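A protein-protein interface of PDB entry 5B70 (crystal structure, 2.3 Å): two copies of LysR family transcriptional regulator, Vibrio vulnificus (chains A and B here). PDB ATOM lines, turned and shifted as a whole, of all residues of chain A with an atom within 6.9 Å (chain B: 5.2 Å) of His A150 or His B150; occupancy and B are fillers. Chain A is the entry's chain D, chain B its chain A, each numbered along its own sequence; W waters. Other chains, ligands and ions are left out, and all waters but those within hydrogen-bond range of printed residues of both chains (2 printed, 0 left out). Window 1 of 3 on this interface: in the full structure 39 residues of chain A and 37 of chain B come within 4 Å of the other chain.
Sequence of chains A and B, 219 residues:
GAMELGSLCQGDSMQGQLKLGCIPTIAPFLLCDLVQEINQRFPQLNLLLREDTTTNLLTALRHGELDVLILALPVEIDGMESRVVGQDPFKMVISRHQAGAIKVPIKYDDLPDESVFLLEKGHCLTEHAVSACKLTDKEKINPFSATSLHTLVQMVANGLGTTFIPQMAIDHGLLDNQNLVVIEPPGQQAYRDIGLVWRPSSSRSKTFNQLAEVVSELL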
ATOM      1  N   PRO A  24      30.992  -6.444  27.738  1.00  0.00           N
ATOM      2  CA  PRO A  24      30.078  -6.168  26.615  1.00  0.00           C
ATOM      3  C   PRO A  24      30.780  -5.923  25.292  1.00  0.00           C
ATOM      4  O   PRO A  24      30.120  -5.974  24.246  1.00  0.00           O
ATOM      5  CB  PRO A  24      29.322  -4.911  27.073  1.00  0.00           C
ATOM      6  CG  PRO A  24      29.482  -4.873  28.550  1.00  0.00           C
ATOM      7  CD  PRO A  24      30.833  -5.460  28.824  1.00  0.00           C
ATOM      8  N   ALA A  27      31.787 -10.163  24.433  1.00  0.00           N
ATOM      9  CA  ALA A  27      30.805 -11.243  24.517  1.00  0.00           C
ATOM     10  C   ALA A  27      29.947 -11.397  23.264  1.00  0.00           C
ATOM     11  O   ALA A  27      29.820 -12.534  22.771  1.00  0.00           O
ATOM     12  CB  ALA A  27      29.938 -11.044  25.767  1.00  0.00           C
ATOM     13  N   PRO A  28      29.344 -10.343  22.696  1.00  0.00           N
ATOM     14  CA  PRO A  28      28.486 -10.552  21.515  1.00  0.00           C
ATOM     15  C   PRO A  28      29.220 -11.093  20.297  1.00  0.00           C
ATOM     16  O   PRO A  28      28.575 -11.694  19.431  1.00  0.00           O
ATOM     17  CB  PRO A  28      27.917  -9.152  21.235  1.00  0.00           C
ATOM     18  CG  PRO A  28      28.082  -8.402  22.510  1.00  0.00           C
ATOM     19  CD  PRO A  28      29.345  -8.927  23.110  1.00  0.00           C
ATOM     20  N   PHE A  29      30.536 -10.913  20.201  1.00  0.00           N
ATOM     21  CA  PHE A  29      31.278 -11.238  18.987  1.00  0.00           C
ATOM     22  C   PHE A  29      32.134 -12.489  19.099  1.00  0.00           C
ATOM     23  O   PHE A  29      32.261 -13.232  18.123  1.00  0.00           O
ATOM     24  CB  PHE A  29      32.166 -10.055  18.589  1.00  0.00           C
ATOM     25  CG  PHE A  29      31.541  -8.717  18.863  1.00  0.00           C
ATOM     26  CD1 PHE A  29      30.520  -8.238  18.060  1.00  0.00           C
ATOM     27  CD2 PHE A  29      31.973  -7.939  19.924  1.00  0.00           C
ATOM     28  CE1 PHE A  29      29.939  -7.007  18.308  1.00  0.00           C
ATOM     29  CE2 PHE A  29      31.398  -6.704  20.178  1.00  0.00           C
ATOM     30  CZ  PHE A  29      30.377  -6.239  19.368  1.00  0.00           C
ATOM     31  N   LEU A  31      31.919 -14.980  21.778  1.00  0.00           N
ATOM     32  CA  LEU A  31      31.288 -16.141  22.389  1.00  0.00           C
ATOM     33  C   LEU A  31      30.411 -16.911  21.413  1.00  0.00           C
ATOM     34  O   LEU A  31      30.119 -18.085  21.661  1.00  0.00           O
ATOM     35  CB  LEU A  31      30.469 -15.715  23.611  1.00  0.00           C
ATOM     36  CG  LEU A  31      31.265 -15.082  24.759  1.00  0.00           C
ATOM     37  CD1 LEU A  31      30.356 -14.710  25.915  1.00  0.00           C
ATOM     38  CD2 LEU A  31      32.381 -16.008  25.232  1.00  0.00           C
ATOM     39  N   CYS A  32      29.990 -16.288  20.310  1.00  0.00           N
ATOM     40  CA  CYS A  32      29.208 -17.015  19.316  1.00  0.00           C
ATOM     41  C   CYS A  32      30.005 -18.181  18.745  1.00  0.00           C
ATOM     42  O   CYS A  32      29.517 -19.316  18.693  1.00  0.00           O
ATOM     43  CB  CYS A  32      28.756 -16.074  18.200  1.00  0.00           C
ATOM     44  SG  CYS A  32      27.449 -14.932  18.685  1.00  0.00           S
ATOM     45  N   LEU A  49      26.536 -17.918  31.071  1.00  0.00           N
ATOM     46  CA  LEU A  49      27.149 -16.657  30.664  1.00  0.00           C
ATOM     47  C   LEU A  49      26.610 -15.456  31.423  1.00  0.00           C
ATOM     48  O   LEU A  49      25.398 -15.297  31.600  1.00  0.00           O
ATOM     49  CB  LEU A  49      26.988 -16.413  29.158  1.00  0.00           C
ATOM     50  CG  LEU A  49      27.541 -17.546  28.293  1.00  0.00           C
ATOM     51  CD1 LEU A  49      26.898 -17.543  26.888  1.00  0.00           C
ATOM     52  CD2 LEU A  49      29.104 -17.404  28.255  1.00  0.00           C
ATOM     53  N   GLU A  51      27.198 -11.261  31.142  1.00  0.00           N
ATOM     54  CA  GLU A  51      27.794 -10.118  30.457  1.00  0.00           C
ATOM     55  C   GLU A  51      27.721  -8.902  31.374  1.00  0.00           C
ATOM     56  O   GLU A  51      26.627  -8.454  31.734  1.00  0.00           O
ATOM     57  CB  GLU A  51      27.093  -9.831  29.126  1.00  0.00           C
ATOM     58  CG  GLU A  51      27.757  -8.727  28.303  1.00  0.00           C
ATOM     59  CD  GLU A  51      26.998  -8.381  27.027  1.00  0.00           C
ATOM     60  OE1 GLU A  51      26.455  -7.257  26.940  1.00  0.00           O
ATOM     61  OE2 GLU A  51      26.951  -9.228  26.107  1.00  0.00           O
ATOM     62  N   LEU A 119      33.019   5.270  24.486  1.00  0.00           N
ATOM     63  CA  LEU A 119      32.091   4.650  25.414  1.00  0.00           C
ATOM     64  C   LEU A 119      32.181   5.308  26.790  1.00  0.00           C
ATOM     65  O   LEU A 119      33.120   6.044  27.108  1.00  0.00           O
ATOM     66  CB  LEU A 119      32.369   3.153  25.539  1.00  0.00           C
ATOM     67  CG  LEU A 119      31.994   2.264  24.354  1.00  0.00           C
ATOM     68  CD1 LEU A 119      32.488   0.843  24.586  1.00  0.00           C
ATOM     69  CD2 LEU A 119      30.490   2.292  24.128  1.00  0.00           C
ATOM     70  N   THR A 147      26.886   4.564  25.699  1.00  0.00           N
ATOM     71  CA  THR A 147      26.642   3.556  26.719  1.00  0.00           C
ATOM     72  C   THR A 147      26.605   2.136  26.168  1.00  0.00           C
ATOM     73  O   THR A 147      26.443   1.192  26.950  1.00  0.00           O
ATOM     74  CB  THR A 147      25.330   3.852  27.460  1.00  0.00           C
ATOM     75  OG1 THR A 147      24.253   3.917  26.520  1.00  0.00           O
ATOM     76  CG2 THR A 147      25.427   5.176  28.193  1.00  0.00           C
ATOM     77  N   SER A 148      26.750   1.955  24.856  1.00  0.00           N
ATOM     78  CA  SER A 148      26.820   0.627  24.258  1.00  0.00           C
ATOM     79  C   SER A 148      27.598   0.714  22.954  1.00  0.00           C
ATOM     80  O   SER A 148      27.656   1.767  22.313  1.00  0.00           O
ATOM     81  CB  SER A 148      25.428   0.035  24.002  1.00  0.00           C
ATOM     82  OG  SER A 148      24.810   0.630  22.872  1.00  0.00           O
ATOM     83  N   LEU A 149      28.192  -0.413  22.558  1.00  0.00           N
ATOM     84  CA  LEU A 149      28.976  -0.418  21.328  1.00  0.00           C
ATOM     85  C   LEU A 149      28.087  -0.304  20.092  1.00  0.00           C
ATOM     86  O   LEU A 149      28.516   0.253  19.075  1.00  0.00           O
ATOM     87  CB  LEU A 149      29.840  -1.677  21.262  1.00  0.00           C
ATOM     88  CG  LEU A 149      30.960  -1.675  20.221  1.00  0.00           C
ATOM     89  CD1 LEU A 149      31.896  -0.504  20.454  1.00  0.00           C
ATOM     90  CD2 LEU A 149      31.728  -2.987  20.252  1.00  0.00           C
ATOM     91  N   HIS A 150      26.851  -0.806  20.160  1.00  0.00           N
ATOM     92  CA  HIS A 150      25.957  -0.728  19.007  1.00  0.00           C
ATOM     93  C   HIS A 150      25.535   0.710  18.735  1.00  0.00           C
ATOM     94  O   HIS A 150      25.602   1.183  17.594  1.00  0.00           O
ATOM     95  CB  HIS A 150      24.731  -1.610  19.226  1.00  0.00           C
ATOM     96  CG  HIS A 150      25.065  -3.032  19.545  1.00  0.00           C
ATOM     97  ND1 HIS A 150      25.303  -3.468  20.829  1.00  0.00           N
ATOM     98  CD2 HIS A 150      25.209  -4.115  18.745  1.00  0.00           C
ATOM     99  CE1 HIS A 150      25.577  -4.761  20.808  1.00  0.00           C
ATOM    100  NE2 HIS A 150      25.527  -5.178  19.555  1.00  0.00           N
ATOM    101  N   THR A 151      25.087   1.418  19.771  1.00  0.00           N
ATOM    102  CA  THR A 151      24.703   2.813  19.595  1.00  0.00           C
ATOM    103  C   THR A 151      25.903   3.692  19.263  1.00  0.00           C
ATOM    104  O   THR A 151      25.741   4.749  18.643  1.00  0.00           O
ATOM    105  CB  THR A 151      24.000   3.319  20.851  1.00  0.00           C
ATOM    106  OG1 THR A 151      24.821   3.052  21.993  1.00  0.00           O
ATOM    107  CG2 THR A 151      22.661   2.619  21.024  1.00  0.00           C
ATOM    108  N   LEU A 152      27.106   3.277  19.667  1.00  0.00           N
ATOM    109  CA  LEU A 152      28.305   4.028  19.315  1.00  0.00           C
ATOM    110  C   LEU A 152      28.559   3.981  17.813  1.00  0.00           C
ATOM    111  O   LEU A 152      28.875   5.006  17.196  1.00  0.00           O
ATOM    112  CB  LEU A 152      29.509   3.478  20.081  1.00  0.00           C
ATOM    113  CG  LEU A 152      30.877   4.082  19.761  1.00  0.00           C
ATOM    114  CD1 LEU A 152      30.886   5.571  20.061  1.00  0.00           C
ATOM    115  CD2 LEU A 152      31.973   3.365  20.534  1.00  0.00           C
ATOM    116  N   VAL A 153      28.423   2.799  17.212  1.00  0.00           N
ATOM    117  CA  VAL A 153      28.578   2.672  15.768  1.00  0.00           C
ATOM    118  C   VAL A 153      27.447   3.388  15.041  1.00  0.00           C
ATOM    119  O   VAL A 153      27.662   4.021  13.999  1.00  0.00           O
ATOM    120  CB  VAL A 153      28.654   1.185  15.377  1.00  0.00           C
ATOM    121  CG1 VAL A 153      28.542   1.022  13.875  1.00  0.00           C
ATOM    122  CG2 VAL A 153      29.949   0.575  15.886  1.00  0.00           C
ATOM    123  N   GLN A 154      26.227   3.311  15.581  1.00  0.00           N
ATOM    124  CA  GLN A 154      25.086   3.944  14.925  1.00  0.00           C
ATOM    125  C   GLN A 154      25.242   5.457  14.857  1.00  0.00           C
ATOM    126  O   GLN A 154      24.809   6.078  13.880  1.00  0.00           O
ATOM    127  CB  GLN A 154      23.791   3.562  15.643  1.00  0.00           C
ATOM    128  CG  GLN A 154      23.412   2.097  15.462  1.00  0.00           C
ATOM    129  CD  GLN A 154      22.484   1.582  16.547  1.00  0.00           C
ATOM    130  OE1 GLN A 154      22.073   2.324  17.439  1.00  0.00           O
ATOM    131  NE2 GLN A 154      22.164   0.296  16.484  1.00  0.00           N
ATOM    132  N   MET A 155      25.860   6.068  15.873  1.00  0.00           N
ATOM    133  CA  MET A 155      26.125   7.504  15.811  1.00  0.00           C
ATOM    134  C   MET A 155      27.188   7.821  14.766  1.00  0.00           C
ATOM    135  O   MET A 155      27.076   8.816  14.040  1.00  0.00           O
ATOM    136  CB  MET A 155      26.544   8.026  17.185  1.00  0.00           C
ATOM    137  CG  MET A 155      25.413   8.083  18.201  1.00  0.00           C
ATOM    138  SD  MET A 155      25.932   8.770  19.785  1.00  0.00           S
ATOM    139  CE  MET A 155      27.167   7.571  20.281  1.00  0.00           C
ATOM    140  N   HIS A 172      32.547  -9.934  13.135  1.00  0.00           N
ATOM    141  CA  HIS A 172      31.214 -10.447  13.419  1.00  0.00           C
ATOM    142  C   HIS A 172      30.131  -9.764  12.592  1.00  0.00           C
ATOM    143  O   HIS A 172      28.999 -10.257  12.554  1.00  0.00           O
ATOM    144  CB  HIS A 172      30.910 -10.294  14.915  1.00  0.00           C
ATOM    145  CG  HIS A 172      29.708 -11.060  15.372  1.00  0.00           C
ATOM    146  ND1 HIS A 172      28.598 -10.447  15.915  1.00  0.00           N
ATOM    147  CD2 HIS A 172      29.443 -12.388  15.371  1.00  0.00           C
ATOM    148  CE1 HIS A 172      27.700 -11.365  16.226  1.00  0.00           C
ATOM    149  NE2 HIS A 172      28.189 -12.551  15.907  1.00  0.00           N
ATOM    150  N   LEU A 174      29.357  -6.195  12.771  1.00  0.00           N
ATOM    151  CA  LEU A 174      28.696  -5.101  13.473  1.00  0.00           C
ATOM    152  C   LEU A 174      28.431  -3.913  12.556  1.00  0.00           C
ATOM    153  O   LEU A 174      27.423  -3.217  12.725  1.00  0.00           O
ATOM    154  CB  LEU A 174      29.545  -4.664  14.665  1.00  0.00           C
ATOM    155  CG  LEU A 174      29.009  -3.499  15.494  1.00  0.00           C
ATOM    156  CD1 LEU A 174      27.705  -3.890  16.166  1.00  0.00           C
ATOM    157  CD2 LEU A 174      30.041  -3.054  16.515  1.00  0.00           C
ATOM    158  N   GLN A 178      25.565  -0.381   7.440  1.00  0.00           N
ATOM    159  CA  GLN A 178      25.581   0.933   8.064  1.00  0.00           C
ATOM    160  C   GLN A 178      26.424   1.933   7.286  1.00  0.00           C
ATOM    161  O   GLN A 178      26.613   3.063   7.750  1.00  0.00           O
ATOM    162  CB  GLN A 178      26.048   0.822   9.515  1.00  0.00           C
ATOM    163  CG  GLN A 178      24.892   0.533  10.462  1.00  0.00           C
ATOM    164  CD  GLN A 178      25.339   0.078  11.828  1.00  0.00           C
ATOM    165  OE1 GLN A 178      26.267  -0.721  11.957  1.00  0.00           O
ATOM    166  NE2 GLN A 178      24.674   0.575  12.861  1.00  0.00           N
ATOM    167  N   PRO B  28      20.103  -2.410  19.419  1.00  0.00           N
ATOM    168  CA  PRO B  28      21.067  -2.991  18.470  1.00  0.00           C
ATOM    169  C   PRO B  28      20.456  -3.421  17.146  1.00  0.00           C
ATOM    170  O   PRO B  28      21.209  -3.728  16.213  1.00  0.00           O
ATOM    171  CB  PRO B  28      21.629  -4.201  19.230  1.00  0.00           C
ATOM    172  CG  PRO B  28      21.286  -3.962  20.660  1.00  0.00           C
ATOM    173  CD  PRO B  28      19.984  -3.241  20.629  1.00  0.00           C
ATOM    174  N   PHE B  29      19.129  -3.445  17.029  1.00  0.00           N
ATOM    175  CA  PHE B  29      18.455  -3.968  15.848  1.00  0.00           C
ATOM    176  C   PHE B  29      17.705  -2.901  15.066  1.00  0.00           C
ATOM    177  O   PHE B  29      17.887  -2.780  13.851  1.00  0.00           O
ATOM    178  CB  PHE B  29      17.490  -5.091  16.265  1.00  0.00           C
ATOM    179  CG  PHE B  29      18.002  -5.938  17.400  1.00  0.00           C
ATOM    180  CD1 PHE B  29      19.015  -6.861  17.195  1.00  0.00           C
ATOM    181  CD2 PHE B  29      17.472  -5.810  18.675  1.00  0.00           C
ATOM    182  CE1 PHE B  29      19.488  -7.641  18.238  1.00  0.00           C
ATOM    183  CE2 PHE B  29      17.942  -6.587  19.722  1.00  0.00           C
ATOM    184  CZ  PHE B  29      18.950  -7.503  19.503  1.00  0.00           C
ATOM    185  N   GLU B  51      21.700   4.005  25.201  1.00  0.00           N
ATOM    186  CA  GLU B  51      21.155   2.674  25.449  1.00  0.00           C
ATOM    187  C   GLU B  51      21.143   2.425  26.952  1.00  0.00           C
ATOM    188  O   GLU B  51      22.199   2.420  27.593  1.00  0.00           O
ATOM    189  CB  GLU B  51      21.967   1.595  24.728  1.00  0.00           C
ATOM    190  CG  GLU B  51      21.306   0.216  24.729  1.00  0.00           C
ATOM    191  CD  GLU B  51      22.151  -0.858  24.053  1.00  0.00           C
ATOM    192  OE1 GLU B  51      22.711  -1.713  24.771  1.00  0.00           O
ATOM    193  OE2 GLU B  51      22.260  -0.845  22.805  1.00  0.00           O
ATOM    194  N   SER B 148      22.220 -10.144  29.087  1.00  0.00           N
ATOM    195  CA  SER B 148      22.202  -9.510  27.777  1.00  0.00           C
ATOM    196  C   SER B 148      21.475 -10.421  26.802  1.00  0.00           C
ATOM    197  O   SER B 148      21.464 -11.646  26.962  1.00  0.00           O
ATOM    198  CB  SER B 148      23.610  -9.215  27.254  1.00  0.00           C
ATOM    199  OG  SER B 148      24.277 -10.413  26.892  1.00  0.00           O
ATOM    200  N   LEU B 149      20.872  -9.808  25.783  1.00  0.00           N
ATOM    201  CA  LEU B 149      20.174 -10.581  24.764  1.00  0.00           C
ATOM    202  C   LEU B 149      21.129 -11.434  23.937  1.00  0.00           C
ATOM    203  O   LEU B 149      20.712 -12.465  23.397  1.00  0.00           O
ATOM    204  CB  LEU B 149      19.375  -9.641  23.860  1.00  0.00           C
ATOM    205  CG  LEU B 149      18.223 -10.258  23.071  1.00  0.00           C
ATOM    206  CD1 LEU B 149      17.273 -10.974  24.011  1.00  0.00           C
ATOM    207  CD2 LEU B 149      17.491  -9.182  22.285  1.00  0.00           C
ATOM    208  N   HIS B 150      22.401 -11.037  23.838  1.00  0.00           N
ATOM    209  CA  HIS B 150      23.378 -11.805  23.073  1.00  0.00           C
ATOM    210  C   HIS B 150      23.825 -13.050  23.826  1.00  0.00           C
ATOM    211  O   HIS B 150      23.839 -14.152  23.263  1.00  0.00           O
ATOM    212  CB  HIS B 150      24.583 -10.928  22.732  1.00  0.00           C
ATOM    213  CG  HIS B 150      24.230  -9.721  21.927  1.00  0.00           C
ATOM    214  ND1 HIS B 150      23.646  -8.603  22.482  1.00  0.00           N
ATOM    215  CD2 HIS B 150      24.350  -9.468  20.602  1.00  0.00           C
ATOM    216  CE1 HIS B 150      23.434  -7.706  21.536  1.00  0.00           C
ATOM    217  NE2 HIS B 150      23.850  -8.206  20.386  1.00  0.00           N
ATOM    218  N   THR B 151      24.205 -12.894  25.097  1.00  0.00           N
ATOM    219  CA  THR B 151      24.612 -14.053  25.886  1.00  0.00           C
ATOM    220  C   THR B 151      23.436 -14.981  26.158  1.00  0.00           C
ATOM    221  O   THR B 151      23.629 -16.192  26.314  1.00  0.00           O
ATOM    222  CB  THR B 151      25.256 -13.606  27.202  1.00  0.00           C
ATOM    223  OG1 THR B 151      24.372 -12.719  27.901  1.00  0.00           O
ATOM    224  CG2 THR B 151      26.576 -12.898  26.934  1.00  0.00           C
ATOM    225  N   LEU B 152      22.217 -14.437  26.213  1.00  0.00           N
ATOM    226  CA  LEU B 152      21.037 -15.285  26.351  1.00  0.00           C
ATOM    227  C   LEU B 152      20.903 -16.228  25.164  1.00  0.00           C
ATOM    228  O   LEU B 152      20.634 -17.423  25.334  1.00  0.00           O
ATOM    229  CB  LEU B 152      19.786 -14.419  26.495  1.00  0.00           C
ATOM    230  CG  LEU B 152      18.438 -15.136  26.560  1.00  0.00           C
ATOM    231  CD1 LEU B 152      18.409 -16.085  27.743  1.00  0.00           C
ATOM    232  CD2 LEU B 152      17.310 -14.120  26.662  1.00  0.00           C
ATOM    233  N   VAL B 153      21.103 -15.709  23.952  1.00  0.00           N
ATOM    234  CA  VAL B 153      21.036 -16.546  22.761  1.00  0.00           C
ATOM    235  C   VAL B 153      22.174 -17.562  22.752  1.00  0.00           C
ATOM    236  O   VAL B 153      21.978 -18.728  22.390  1.00  0.00           O
ATOM    237  CB  VAL B 153      21.046 -15.662  21.500  1.00  0.00           C
ATOM    238  CG1 VAL B 153      21.278 -16.500  20.260  1.00  0.00           C
ATOM    239  CG2 VAL B 153      19.738 -14.891  21.388  1.00  0.00           C
ATOM    240  N   GLN B 154      23.376 -17.142  23.157  1.00  0.00           N
ATOM    241  CA  GLN B 154      24.525 -18.043  23.129  1.00  0.00           C
ATOM    242  C   GLN B 154      24.344 -19.223  24.078  1.00  0.00           C
ATOM    243  O   GLN B 154      24.809 -20.331  23.783  1.00  0.00           O
ATOM    244  CB  GLN B 154      25.804 -17.271  23.465  1.00  0.00           C
ATOM    245  CG  GLN B 154      26.209 -16.231  22.422  1.00  0.00           C
ATOM    246  CD  GLN B 154      27.058 -15.116  23.013  1.00  0.00           C
ATOM    247  OE1 GLN B 154      27.251 -15.049  24.227  1.00  0.00           O
ATOM    248  NE2 GLN B 154      27.551 -14.225  22.156  1.00  0.00           N
ATOM    249  N   LEU B 174      20.612 -11.890  14.672  1.00  0.00           N
ATOM    250  CA  LEU B 174      21.179 -12.303  15.950  1.00  0.00           C
ATOM    251  C   LEU B 174      21.454 -13.800  16.011  1.00  0.00           C
ATOM    252  O   LEU B 174      22.327 -14.225  16.774  1.00  0.00           O
ATOM    253  CB  LEU B 174      20.249 -11.897  17.093  1.00  0.00           C
ATOM    254  CG  LEU B 174      20.744 -12.107  18.525  1.00  0.00           C
ATOM    255  CD1 LEU B 174      22.037 -11.341  18.759  1.00  0.00           C
ATOM    256  CD2 LEU B 174      19.681 -11.684  19.524  1.00  0.00           C
HETATM  257  O   HOH W   1      24.785 -12.371  16.517  1.00  0.00           O
HETATM  258  O   HOH W   2      24.459 -14.350  20.178  1.00  0.00           O
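O of Glu B51 sits at hydrogen-bond distance from OG1 of Thr A147 (2.8 Å).
The side-chain hydroxyl of Ser A148 lies within hydrogen-bond range of the side-chain carboxylate of Glu B51 (2.9 Å).
The side-chain hydroxyl of Ser B148 is in hydrogen-bond range of the side-chain carboxylate of Glu A51 (3.0 Å).
The backbone carbonyl oxygen (O) of Ala A27 lies within hydrogen-bond range of the side-chain amide nitrogen (NE2) of Gln B154 (2.9 Å).
The side-chain sulfur of Cys A32 is in hydrogen-bond range of the side-chain amide nitrogen of Gln B154 (3.5 Å).
OG of Ser B148 is in hydrogen-bond range of OG1 of Thr B151 (2.5 Å).
The backbone carbonyl oxygen of Pro A28 lies within hydrogen-bond range of the side-chain sulfur of Cys A32.
The side-chain sulfur (SG) of Cys A32 lies within hydrogen-bond range of a ring nitrogen (NE2) of His A172 (3.7 Å).
OG of Ser A148 is in hydrogen-bond range of OG1 of Thr A151 (2.6 Å).
Among the printed residues, pairs that only touch across the chains: Leu A31 with Gln B154 (3.3 Å), His A150 with His B150 (3.6 Å), Leu A49 with Thr B151 (3.6 Å), Leu A49 with Gln B154 (3.6 Å), His A150 with Pro B28 (3.6 Å), Pro A28 with His B150 (3.6 Å), Glu A51 with Thr B151 (3.8 Å), Pro A28 with Gln B154 (3.8 Å), Thr A151 with Glu B51 (3.9 Å) and Gln A154 with Pro B28 (3.99 Å).
Printed residues of chain B within 4 Å of Ser A148: Glu B51 (2.9 Å).
Of chain B, only Pro B28 (3.6 Å) and His B150 (3.6 Å) come within 4 Å of His A150.
Of the printed residues of chain A, Ser B148 touches Glu A51 (3.0 Å).
Of the printed residues of chain A, Thr B151 touches Leu A49 (3.6 Å) and Glu A51 (3.8 Å).
The nearest residue of chain B that does not touch His A150 is Glu B51 (4.4 Å).
The nearest printed residue of chain B that does not touch Thr A151 is Pro B28 (5.9 Å).
Of the 11 printed residues of chain B, 6 touch a printed residue of chain A.
Hydrophobic or aromatic side chains of chain B within 4 Å of the printed part of chain A: Pro B28 and His B150.
Of the 21 printed residues of chain A, 11 touch a printed residue of chain B.
Pro A28 touches His B150, and with the chains exchanged His A150 touches Pro B28.
Pro A28 touches Gln B154, and with the chains exchanged Gln A154 touches Pro B28.
Glu A51 touches Thr B151, and with the chains exchanged Thr A151 touches Glu B51.
His A150 touches its own counterpart, His B150.
Positions printed for both chains: 28, 29, 51, 148, 149, 150, 151, 152, 153, 154 and 174.
Of the 15 pairs that touch across the chains among the printed residues, 9 have their exchanged pair printed and touching as well.
Water W1 bridges O of Leu B174 and NE2 of His A172.
Water W2 lies within hydrogen-bond range of O of His B150 (3.2 Å) and SG of Cys A32 (3.4 Å).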
